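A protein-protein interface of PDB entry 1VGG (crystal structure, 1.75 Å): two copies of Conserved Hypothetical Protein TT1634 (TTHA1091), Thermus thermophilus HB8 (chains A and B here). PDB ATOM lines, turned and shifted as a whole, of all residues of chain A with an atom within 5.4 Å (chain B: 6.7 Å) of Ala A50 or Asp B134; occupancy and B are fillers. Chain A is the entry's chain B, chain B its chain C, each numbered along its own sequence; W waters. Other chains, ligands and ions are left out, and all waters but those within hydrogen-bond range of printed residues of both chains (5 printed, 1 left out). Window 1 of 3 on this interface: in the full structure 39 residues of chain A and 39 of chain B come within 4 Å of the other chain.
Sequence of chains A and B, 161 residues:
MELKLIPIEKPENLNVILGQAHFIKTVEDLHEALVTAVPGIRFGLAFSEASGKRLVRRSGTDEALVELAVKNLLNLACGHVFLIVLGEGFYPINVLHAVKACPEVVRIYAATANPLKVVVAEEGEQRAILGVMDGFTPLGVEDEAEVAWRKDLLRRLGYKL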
ATOM      1  N   GLN A  20      19.637 -36.915  25.505  1.00  0.00           N
ATOM      2  CA  GLN A  20      20.700 -36.083  24.949  1.00  0.00           C
ATOM      3  C   GLN A  20      21.957 -36.946  24.805  1.00  0.00           C
ATOM      4  O   GLN A  20      22.327 -37.682  25.723  1.00  0.00           O
ATOM      5  CB  GLN A  20      20.976 -34.919  25.904  1.00  0.00           C
ATOM      6  CG  GLN A  20      21.931 -33.850  25.389  1.00  0.00           C
ATOM      7  CD  GLN A  20      21.296 -32.931  24.375  1.00  0.00           C
ATOM      8  OE1 GLN A  20      20.084 -32.691  24.401  1.00  0.00           O
ATOM      9  NE2 GLN A  20      22.117 -32.388  23.478  1.00  0.00           N
ATOM     10  N   ALA A  21      22.603 -36.864  23.648  1.00  0.00           N
ATOM     11  CA  ALA A  21      23.824 -37.630  23.404  1.00  0.00           C
ATOM     12  C   ALA A  21      24.820 -36.732  22.660  1.00  0.00           C
ATOM     13  O   ALA A  21      24.679 -35.506  22.659  1.00  0.00           O
ATOM     14  CB  ALA A  21      23.505 -38.887  22.567  1.00  0.00           C
ATOM     15  N   HIS A  22      25.838 -37.342  22.064  1.00  0.00           N
ATOM     16  CA  HIS A  22      26.844 -36.611  21.287  1.00  0.00           C
ATOM     17  C   HIS A  22      27.665 -37.647  20.515  1.00  0.00           C
ATOM     18  O   HIS A  22      27.641 -38.828  20.858  1.00  0.00           O
ATOM     19  CB  HIS A  22      27.751 -35.778  22.209  1.00  0.00           C
ATOM     20  CG  HIS A  22      28.820 -36.571  22.893  1.00  0.00           C
ATOM     21  ND1 HIS A  22      28.540 -37.591  23.774  1.00  0.00           N
ATOM     22  CD2 HIS A  22      30.172 -36.503  22.811  1.00  0.00           C
ATOM     23  CE1 HIS A  22      29.672 -38.121  24.207  1.00  0.00           C
ATOM     24  NE2 HIS A  22      30.677 -37.479  23.636  1.00  0.00           N
ATOM     25  N   SER A  48      19.919 -36.529  16.321  1.00  0.00           N
ATOM     26  CA  SER A  48      20.104 -35.284  15.575  1.00  0.00           C
ATOM     27  C   SER A  48      21.547 -34.767  15.605  1.00  0.00           C
ATOM     28  O   SER A  48      21.981 -34.164  16.585  1.00  0.00           O
ATOM     29  CB  SER A  48      19.140 -34.218  16.129  1.00  0.00           C
ATOM     30  OG  SER A  48      18.820 -33.213  15.172  1.00  0.00           O
ATOM     31  N   GLU A  49      22.285 -35.019  14.524  1.00  0.00           N
ATOM     32  CA  GLU A  49      23.668 -34.567  14.392  1.00  0.00           C
ATOM     33  C   GLU A  49      23.627 -33.046  14.543  1.00  0.00           C
ATOM     34  O   GLU A  49      22.890 -32.373  13.829  1.00  0.00           O
ATOM     35  CB  GLU A  49      24.197 -34.965  13.013  1.00  0.00           C
ATOM     36  CG  GLU A  49      25.669 -34.717  12.800  1.00  0.00           C
ATOM     37  CD  GLU A  49      26.107 -35.077  11.385  1.00  0.00           C
ATOM     38  OE1 GLU A  49      27.328 -35.131  11.132  1.00  0.00           O
ATOM     39  OE2 GLU A  49      25.229 -35.296  10.527  1.00  0.00           O
ATOM     40  N   ALA A  50      24.433 -32.511  15.460  1.00  0.00           N
ATOM     41  CA  ALA A  50      24.417 -31.082  15.765  1.00  0.00           C
ATOM     42  C   ALA A  50      25.363 -30.192  14.973  1.00  0.00           C
ATOM     43  O   ALA A  50      25.261 -28.963  15.036  1.00  0.00           O
ATOM     44  CB  ALA A  50      24.652 -30.885  17.269  1.00  0.00           C
ATOM     45  N   SER A  51      26.275 -30.800  14.229  1.00  0.00           N
ATOM     46  CA  SER A  51      27.227 -30.036  13.425  1.00  0.00           C
ATOM     47  C   SER A  51      27.488 -30.748  12.113  1.00  0.00           C
ATOM     48  O   SER A  51      26.772 -31.678  11.759  1.00  0.00           O
ATOM     49  CB  SER A  51      28.544 -29.852  14.179  1.00  0.00           C
ATOM     50  OG  SER A  51      28.378 -28.988  15.284  1.00  0.00           O
ATOM     51  N   GLY A  52      28.522 -30.319  11.395  1.00  0.00           N
ATOM     52  CA  GLY A  52      28.813 -30.944  10.117  1.00  0.00           C
ATOM     53  C   GLY A  52      27.637 -30.741   9.175  1.00  0.00           C
ATOM     54  O   GLY A  52      27.169 -29.618   8.996  1.00  0.00           O
ATOM     55  N   ARG A  54      24.746 -31.720   9.743  1.00  0.00           N
ATOM     56  CA  ARG A  54      23.555 -31.585  10.594  1.00  0.00           C
ATOM     57  C   ARG A  54      22.390 -32.454  10.131  1.00  0.00           C
ATOM     58  O   ARG A  54      21.262 -31.989   9.992  1.00  0.00           O
ATOM     59  CB  ARG A  54      23.123 -30.108  10.638  1.00  0.00           C
ATOM     60  CG  ARG A  54      24.162 -29.193  11.304  1.00  0.00           C
ATOM     61  CD  ARG A  54      24.018 -27.733  10.882  1.00  0.00           C
ATOM     62  NE  ARG A  54      22.704 -27.175  11.197  1.00  0.00           N
ATOM     63  CZ  ARG A  54      22.343 -25.923  10.936  1.00  0.00           C
ATOM     64  NH1 ARG A  54      21.128 -25.498  11.256  1.00  0.00           N
ATOM     65  NH2 ARG A  54      23.193 -25.092  10.350  1.00  0.00           N
ATOM     66  N   CYS A  78      16.335 -30.273  17.588  1.00  0.00           N
ATOM     67  CA  CYS A  78      17.275 -29.892  18.645  1.00  0.00           C
ATOM     68  C   CYS A  78      18.585 -30.653  18.472  1.00  0.00           C
ATOM     69  O   CYS A  78      18.591 -31.884  18.459  1.00  0.00           O
ATOM     70  CB  CYS A  78      16.706 -30.242  20.031  1.00  0.00           C
ATOM     71  SG  CYS A  78      15.283 -29.278  20.626  1.00  0.00           S
ATOM     72  N   GLY A  79      19.697 -29.933  18.359  1.00  0.00           N
ATOM     73  CA  GLY A  79      20.972 -30.605  18.201  1.00  0.00           C
ATOM     74  C   GLY A  79      21.288 -31.588  19.323  1.00  0.00           C
ATOM     75  O   GLY A  79      21.062 -31.292  20.495  1.00  0.00           O
ATOM     76  N   HIS A  80      21.795 -32.759  18.933  1.00  0.00           N
ATOM     77  CA  HIS A  80      22.210 -33.840  19.831  1.00  0.00           C
ATOM     78  C   HIS A  80      21.137 -34.584  20.623  1.00  0.00           C
ATOM     79  O   HIS A  80      21.452 -35.377  21.511  1.00  0.00           O
ATOM     80  CB  HIS A  80      23.318 -33.336  20.772  1.00  0.00           C
ATOM     81  CG  HIS A  80      24.693 -33.410  20.173  1.00  0.00           C
ATOM     82  ND1 HIS A  80      25.799 -32.843  20.767  1.00  0.00           N
ATOM     83  CD2 HIS A  80      25.137 -33.990  19.030  1.00  0.00           C
ATOM     84  CE1 HIS A  80      26.865 -33.063  20.017  1.00  0.00           C
ATOM     85  NE2 HIS A  80      26.490 -33.759  18.956  1.00  0.00           N
ATOM     86  N   GLN A 126      19.455 -22.686  16.627  1.00  0.00           N
ATOM     87  CA  GLN A 126      19.725 -23.528  17.789  1.00  0.00           C
ATOM     88  C   GLN A 126      18.468 -23.670  18.619  1.00  0.00           C
ATOM     89  O   GLN A 126      17.697 -22.719  18.761  1.00  0.00           O
ATOM     90  CB  GLN A 126      20.790 -22.916  18.694  1.00  0.00           C
ATOM     91  CG  GLN A 126      22.200 -22.962  18.177  1.00  0.00           C
ATOM     92  CD  GLN A 126      23.196 -22.665  19.278  1.00  0.00           C
ATOM     93  OE1 GLN A 126      23.311 -21.526  19.745  1.00  0.00           O
ATOM     94  NE2 GLN A 126      23.918 -23.694  19.713  1.00  0.00           N
ATOM     95  N   ARG A 127      18.267 -24.861  19.170  1.00  0.00           N
ATOM     96  CA  ARG A 127      17.136 -25.126  20.039  1.00  0.00           C
ATOM     97  C   ARG A 127      17.628 -25.921  21.244  1.00  0.00           C
ATOM     98  O   ARG A 127      18.607 -26.660  21.151  1.00  0.00           O
ATOM     99  CB  ARG A 127      16.042 -25.889  19.290  1.00  0.00           C
ATOM    100  CG  ARG A 127      15.155 -24.954  18.471  1.00  0.00           C
ATOM    101  CD  ARG A 127      14.584 -25.594  17.219  1.00  0.00           C
ATOM    102  NE  ARG A 127      13.501 -26.536  17.485  1.00  0.00           N
ATOM    103  CZ  ARG A 127      12.221 -26.323  17.186  1.00  0.00           C
ATOM    104  NH1 ARG A 127      11.318 -27.249  17.460  1.00  0.00           N
ATOM    105  NH2 ARG A 127      11.839 -25.191  16.615  1.00  0.00           N
ATOM    106  N   TYR B 109      24.227 -32.069  31.875  1.00  0.00           N
ATOM    107  CA  TYR B 109      23.430 -31.292  30.920  1.00  0.00           C
ATOM    108  C   TYR B 109      23.875 -31.484  29.489  1.00  0.00           C
ATOM    109  O   TYR B 109      23.047 -31.626  28.591  1.00  0.00           O
ATOM    110  CB  TYR B 109      23.505 -29.798  31.240  1.00  0.00           C
ATOM    111  CG  TYR B 109      22.927 -29.431  32.580  1.00  0.00           C
ATOM    112  CD1 TYR B 109      21.564 -29.559  32.819  1.00  0.00           C
ATOM    113  CD2 TYR B 109      23.737 -28.950  33.610  1.00  0.00           C
ATOM    114  CE1 TYR B 109      21.015 -29.215  34.045  1.00  0.00           C
ATOM    115  CE2 TYR B 109      23.192 -28.602  34.854  1.00  0.00           C
ATOM    116  CZ  TYR B 109      21.828 -28.740  35.052  1.00  0.00           C
ATOM    117  OH  TYR B 109      21.251 -28.401  36.257  1.00  0.00           O
ATOM    118  N   ALA B 110      25.185 -31.485  29.275  1.00  0.00           N
ATOM    119  CA  ALA B 110      25.709 -31.631  27.929  1.00  0.00           C
ATOM    120  C   ALA B 110      27.157 -32.092  27.918  1.00  0.00           C
ATOM    121  O   ALA B 110      27.892 -31.890  28.878  1.00  0.00           O
ATOM    122  CB  ALA B 110      25.592 -30.295  27.184  1.00  0.00           C
ATOM    123  N   ALA B 111      27.546 -32.735  26.820  1.00  0.00           N
ATOM    124  CA  ALA B 111      28.919 -33.202  26.619  1.00  0.00           C
ATOM    125  C   ALA B 111      29.079 -32.927  25.135  1.00  0.00           C
ATOM    126  O   ALA B 111      28.358 -33.504  24.331  1.00  0.00           O
ATOM    127  CB  ALA B 111      29.029 -34.702  26.909  1.00  0.00           C
ATOM    128  N   THR B 112      30.010 -32.059  24.755  1.00  0.00           N
ATOM    129  CA  THR B 112      30.086 -31.719  23.341  1.00  0.00           C
ATOM    130  C   THR B 112      31.331 -30.960  22.927  1.00  0.00           C
ATOM    131  O   THR B 112      32.046 -30.400  23.752  1.00  0.00           O
ATOM    132  CB  THR B 112      28.849 -30.859  22.961  1.00  0.00           C
ATOM    133  OG1 THR B 112      28.801 -30.644  21.542  1.00  0.00           O
ATOM    134  CG2 THR B 112      28.913 -29.510  23.676  1.00  0.00           C
ATOM    135  N   ALA B 113      31.563 -30.947  21.619  1.00  0.00           N
ATOM    136  CA  ALA B 113      32.683 -30.239  21.023  1.00  0.00           C
ATOM    137  C   ALA B 113      32.131 -29.111  20.138  1.00  0.00           C
ATOM    138  O   ALA B 113      32.894 -28.370  19.517  1.00  0.00           O
ATOM    139  CB  ALA B 113      33.516 -31.204  20.192  1.00  0.00           C
ATOM    140  N   ASN B 114      30.805 -28.981  20.098  1.00  0.00           N
ATOM    141  CA  ASN B 114      30.132 -27.957  19.284  1.00  0.00           C
ATOM    142  C   ASN B 114      29.841 -26.692  20.075  1.00  0.00           C
ATOM    143  O   ASN B 114      29.943 -26.688  21.300  1.00  0.00           O
ATOM    144  CB  ASN B 114      28.790 -28.479  18.778  1.00  0.00           C
ATOM    145  CG  ASN B 114      28.910 -29.788  18.061  1.00  0.00           C
ATOM    146  OD1 ASN B 114      28.118 -30.700  18.290  1.00  0.00           O
ATOM    147  ND2 ASN B 114      29.897 -29.895  17.180  1.00  0.00           N
ATOM    148  N   PRO B 115      29.453 -25.602  19.382  1.00  0.00           N
ATOM    149  CA  PRO B 115      29.139 -24.341  20.059  1.00  0.00           C
ATOM    150  C   PRO B 115      27.975 -24.595  21.003  1.00  0.00           C
ATOM    151  O   PRO B 115      26.977 -25.220  20.632  1.00  0.00           O
ATOM    152  CB  PRO B 115      28.765 -23.412  18.904  1.00  0.00           C
ATOM    153  CG  PRO B 115      29.653 -23.902  17.811  1.00  0.00           C
ATOM    154  CD  PRO B 115      29.467 -25.404  17.921  1.00  0.00           C
ATOM    155  N   LEU B 116      28.104 -24.088  22.219  1.00  0.00           N
ATOM    156  CA  LEU B 116      27.110 -24.305  23.260  1.00  0.00           C
ATOM    157  C   LEU B 116      26.648 -23.025  23.945  1.00  0.00           C
ATOM    158  O   LEU B 116      27.457 -22.140  24.225  1.00  0.00           O
ATOM    159  CB  LEU B 116      27.734 -25.240  24.302  1.00  0.00           C
ATOM    160  CG  LEU B 116      27.021 -25.663  25.579  1.00  0.00           C
ATOM    161  CD1 LEU B 116      25.789 -26.496  25.242  1.00  0.00           C
ATOM    162  CD2 LEU B 116      27.999 -26.467  26.423  1.00  0.00           C
ATOM    163  N   LYS B 117      25.344 -22.937  24.209  1.00  0.00           N
ATOM    164  CA  LYS B 117      24.756 -21.806  24.917  1.00  0.00           C
ATOM    165  C   LYS B 117      23.858 -22.394  25.995  1.00  0.00           C
ATOM    166  O   LYS B 117      23.258 -23.454  25.800  1.00  0.00           O
ATOM    167  CB  LYS B 117      23.928 -20.918  23.986  1.00  0.00           C
ATOM    168  CG  LYS B 117      24.747 -20.198  22.939  1.00  0.00           C
ATOM    169  CD  LYS B 117      23.905 -19.167  22.198  1.00  0.00           C
ATOM    170  CE  LYS B 117      24.721 -18.459  21.132  1.00  0.00           C
ATOM    171  NZ  LYS B 117      23.914 -17.411  20.437  1.00  0.00           N
ATOM    172  N   VAL B 132      20.308 -26.633  27.415  1.00  0.00           N
ATOM    173  CA  VAL B 132      21.495 -26.263  26.671  1.00  0.00           C
ATOM    174  C   VAL B 132      21.229 -26.287  25.174  1.00  0.00           C
ATOM    175  O   VAL B 132      20.584 -27.201  24.655  1.00  0.00           O
ATOM    176  CB  VAL B 132      22.669 -27.229  26.981  1.00  0.00           C
ATOM    177  CG1 VAL B 132      23.069 -27.133  28.460  1.00  0.00           C
ATOM    178  CG2 VAL B 132      22.266 -28.657  26.650  1.00  0.00           C
ATOM    179  N   MET B 133      21.693 -25.254  24.489  1.00  0.00           N
ATOM    180  CA  MET B 133      21.571 -25.198  23.036  1.00  0.00           C
ATOM    181  C   MET B 133      22.910 -25.775  22.589  1.00  0.00           C
ATOM    182  O   MET B 133      23.928 -25.082  22.583  1.00  0.00           O
ATOM    183  CB  MET B 133      21.412 -23.752  22.571  1.00  0.00           C
ATOM    184  CG  MET B 133      20.063 -23.172  22.935  1.00  0.00           C
ATOM    185  SD  MET B 133      19.784 -21.436  22.135  1.00  0.00           S
ATOM    186  CE  MET B 133      18.032 -21.048  22.889  1.00  0.00           C
ATOM    187  N   ASP B 134      22.897 -27.060  22.258  1.00  0.00           N
ATOM    188  CA  ASP B 134      24.094 -27.797  21.862  1.00  0.00           C
ATOM    189  C   ASP B 134      24.129 -27.963  20.357  1.00  0.00           C
ATOM    190  O   ASP B 134      23.418 -28.796  19.788  1.00  0.00           O
ATOM    191  CB  ASP B 134      24.080 -29.173  22.547  1.00  0.00           C
ATOM    192  CG  ASP B 134      25.326 -29.996  22.257  1.00  0.00           C
ATOM    193  OD1 ASP B 134      25.388 -31.153  22.732  1.00  0.00           O
ATOM    194  OD2 ASP B 134      26.237 -29.492  21.569  1.00  0.00           O
ATOM    195  N   GLY B 135      24.952 -27.169  19.699  1.00  0.00           N
ATOM    196  CA  GLY B 135      24.993 -27.305  18.264  1.00  0.00           C
ATOM    197  C   GLY B 135      23.740 -26.746  17.630  1.00  0.00           C
ATOM    198  O   GLY B 135      22.974 -25.999  18.252  1.00  0.00           O
ATOM    199  N   PHE B 136      23.506 -27.172  16.397  1.00  0.00           N
ATOM    200  CA  PHE B 136      22.426 -26.638  15.589  1.00  0.00           C
ATOM    201  C   PHE B 136      21.286 -27.549  15.175  1.00  0.00           C
ATOM    202  O   PHE B 136      21.346 -28.765  15.325  1.00  0.00           O
ATOM    203  CB  PHE B 136      23.104 -26.002  14.371  1.00  0.00           C
ATOM    204  CG  PHE B 136      24.280 -25.145  14.755  1.00  0.00           C
ATOM    205  CD1 PHE B 136      24.081 -23.862  15.261  1.00  0.00           C
ATOM    206  CD2 PHE B 136      25.572 -25.666  14.749  1.00  0.00           C
ATOM    207  CE1 PHE B 136      25.147 -23.112  15.764  1.00  0.00           C
ATOM    208  CE2 PHE B 136      26.648 -24.924  15.252  1.00  0.00           C
ATOM    209  CZ  PHE B 136      26.430 -23.643  15.763  1.00  0.00           C
ATOM    210  N   THR B 137      20.234 -26.925  14.660  1.00  0.00           N
ATOM    211  CA  THR B 137      19.046 -27.627  14.208  1.00  0.00           C
ATOM    212  C   THR B 137      19.393 -28.465  12.988  1.00  0.00           C
ATOM    213  O   THR B 137      20.351 -28.172  12.269  1.00  0.00           O
ATOM    214  CB  THR B 137      17.929 -26.625  13.853  1.00  0.00           C
ATOM    215  OG1 THR B 137      18.407 -25.714  12.855  1.00  0.00           O
ATOM    216  CG2 THR B 137      17.516 -25.841  15.091  1.00  0.00           C
HETATM  217  O   HOH W   1      20.644 -31.305  14.651  1.00  0.00           O
HETATM  218  O   HOH W   2      21.919 -19.435  19.102  1.00  0.00           O
HETATM  219  O   HOH W   3      18.879 -29.578  24.302  1.00  0.00           O
HETATM  220  O   HOH W   4      25.274 -33.119  24.733  1.00  0.00           O
HETATM  221  O   HOH W   5      20.252 -27.008  18.715  1.00  0.00           O
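NE of Arg A54 lies within hydrogen-bond range of O of Thr B137.
NE2 of Gln A126 sits at hydrogen-bond distance from O of Met B133 (3.2 Å).
OD1 of Asp B134 sits at hydrogen-bond distance from ND1 of His A80 (2.6 Å).
The side-chain amide nitrogen (ND2) of Asn B114 lies within hydrogen-bond range of the side-chain hydroxyl (OG) of Ser A51 (2.6 Å).
The backbone carbonyl oxygen of Ala A50 sits at hydrogen-bond distance from the backbone NH of Phe B136 (2.9 Å).
The backbone carbonyl oxygen (O) of Gly B135 lies within hydrogen-bond range of the side-chain amide nitrogen (NE2) of Gln A126 (2.9 Å).
The side-chain hydroxyl (OG1) of Thr B112 is in hydrogen-bond range of the side-chain carboxylate (OD2) of Asp B134.
O of Pro B115 sits at hydrogen-bond distance from N of Gly B135, at 3.0 Å.
O of Lys B117 is in hydrogen-bond range of N of Met B133, at 2.7 Å.
N of Ala A21 lies within hydrogen-bond range of O of His A80 (2.8 Å).
N of Asn B114 lies within hydrogen-bond range of OG1 of Thr B112, 3.0 Å away.
The backbone NH (N) of His A80 lies within hydrogen-bond range of the backbone carbonyl oxygen (O) of Ser A48 (2.7 Å).
Among the printed residues, pairs that only touch across the chains: His A22 with Ala B111, His A80 with Asn B114, Arg A54 with Phe B136, Gly A79 with Asp B134, Gly A79 with Phe B136, His A80 with Thr B112, Gln A126 with Lys B117, Ala A50 with Asp B134, Gln A126 with Pro B115, Gln A20 with Asp B134, Gln A126 with Phe B136, Ala A50 with Asn B114, Arg A127 with Thr B137, Ala A50 with Gly B135 and Arg A127 with Met B133.
Of chain A, only Gln A20, Ala A50, Gly A79 and His A80 come within 4 Å of Asp B134.
Of the printed residues of chain B, Gln A126 touches Pro B115, Lys B117, Met B133, Gly B135 and Phe B136.
Printed residues of chain A within 4 Å of Gly B135: Ala A50 and Gln A126.
Of the printed residues of chain B, His A80 touches Thr B112 (3.5 Å), Asn B114 (3.2 Å) and Asp B134 (2.6 Å).
Of the printed residues of chain B, Arg A127 touches Met B133 and Thr B137.
Of the printed residues of chain B, Gly A79 touches Asp B134 (3.4 Å) and Phe B136 (3.4 Å).
Tyr B109 touches none of the printed residues of chain A.
Ala B113 touches none of the printed residues of chain A.
The nearest printed residue of chain B that does not touch Arg A127 is Val B132 (4.1 Å).
Printed residues of chain A that touch a printed residue of chain B: Gln A20, His A22, Ala A50, Ser A51, Arg A54, Gly A79, His A80, Gln A126 and Arg A127.
Hydrophobic or aromatic side chains of chain A that line the printed part of chain B: His A22, Ala A50 and His A80.
Printed residues of chain B that touch a printed residue of chain A: Ala B111, Thr B112, Asn B114, Pro B115, Lys B117, Met B133, Asp B134, Gly B135, Phe B136 and Thr B137.
Hydrophobic or aromatic side chains of chain B within 4 Å of the printed part of chain A: Met B133 and Phe B136.
Among the printed residues, 21 pairs touch across the chains.
Among the printed residues, no Asp or Glu carboxylate lies within 4 Å of a Lys or Arg side-chain nitrogen of the other chain.
No position is printed for both chains.
Of the 21 pairs that touch across the chains among the printed residues, none has its exchanged pair printed and touching as well.
Water W2 bridges OE1 of Gln A126 (2.6 Å) and NZ of Lys B117 (3.1 Å).
Water W1 lies within hydrogen-bond range of O of Glu A49 (2.6 Å), OG of Ser A48 (2.7 Å) and O of Phe B136 (2.7 Å).
Water W4 lies within hydrogen-bond range of the side-chain carboxylate of Asp B134, the backbone NH of Ala B111, the backbone carbonyl oxygen of Ala A21 and the side-chain amide nitrogen of Gln A20.
Water W5 lies within hydrogen-bond range of the backbone carbonyl oxygen (O) of Gly B135, the backbone NH (N) of Arg A127 and the backbone NH (N) of Gly A79.
Water W3 bridges O of Val B132 (2.9 Å) and OE1 of Gln A20 (3.3 Å).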
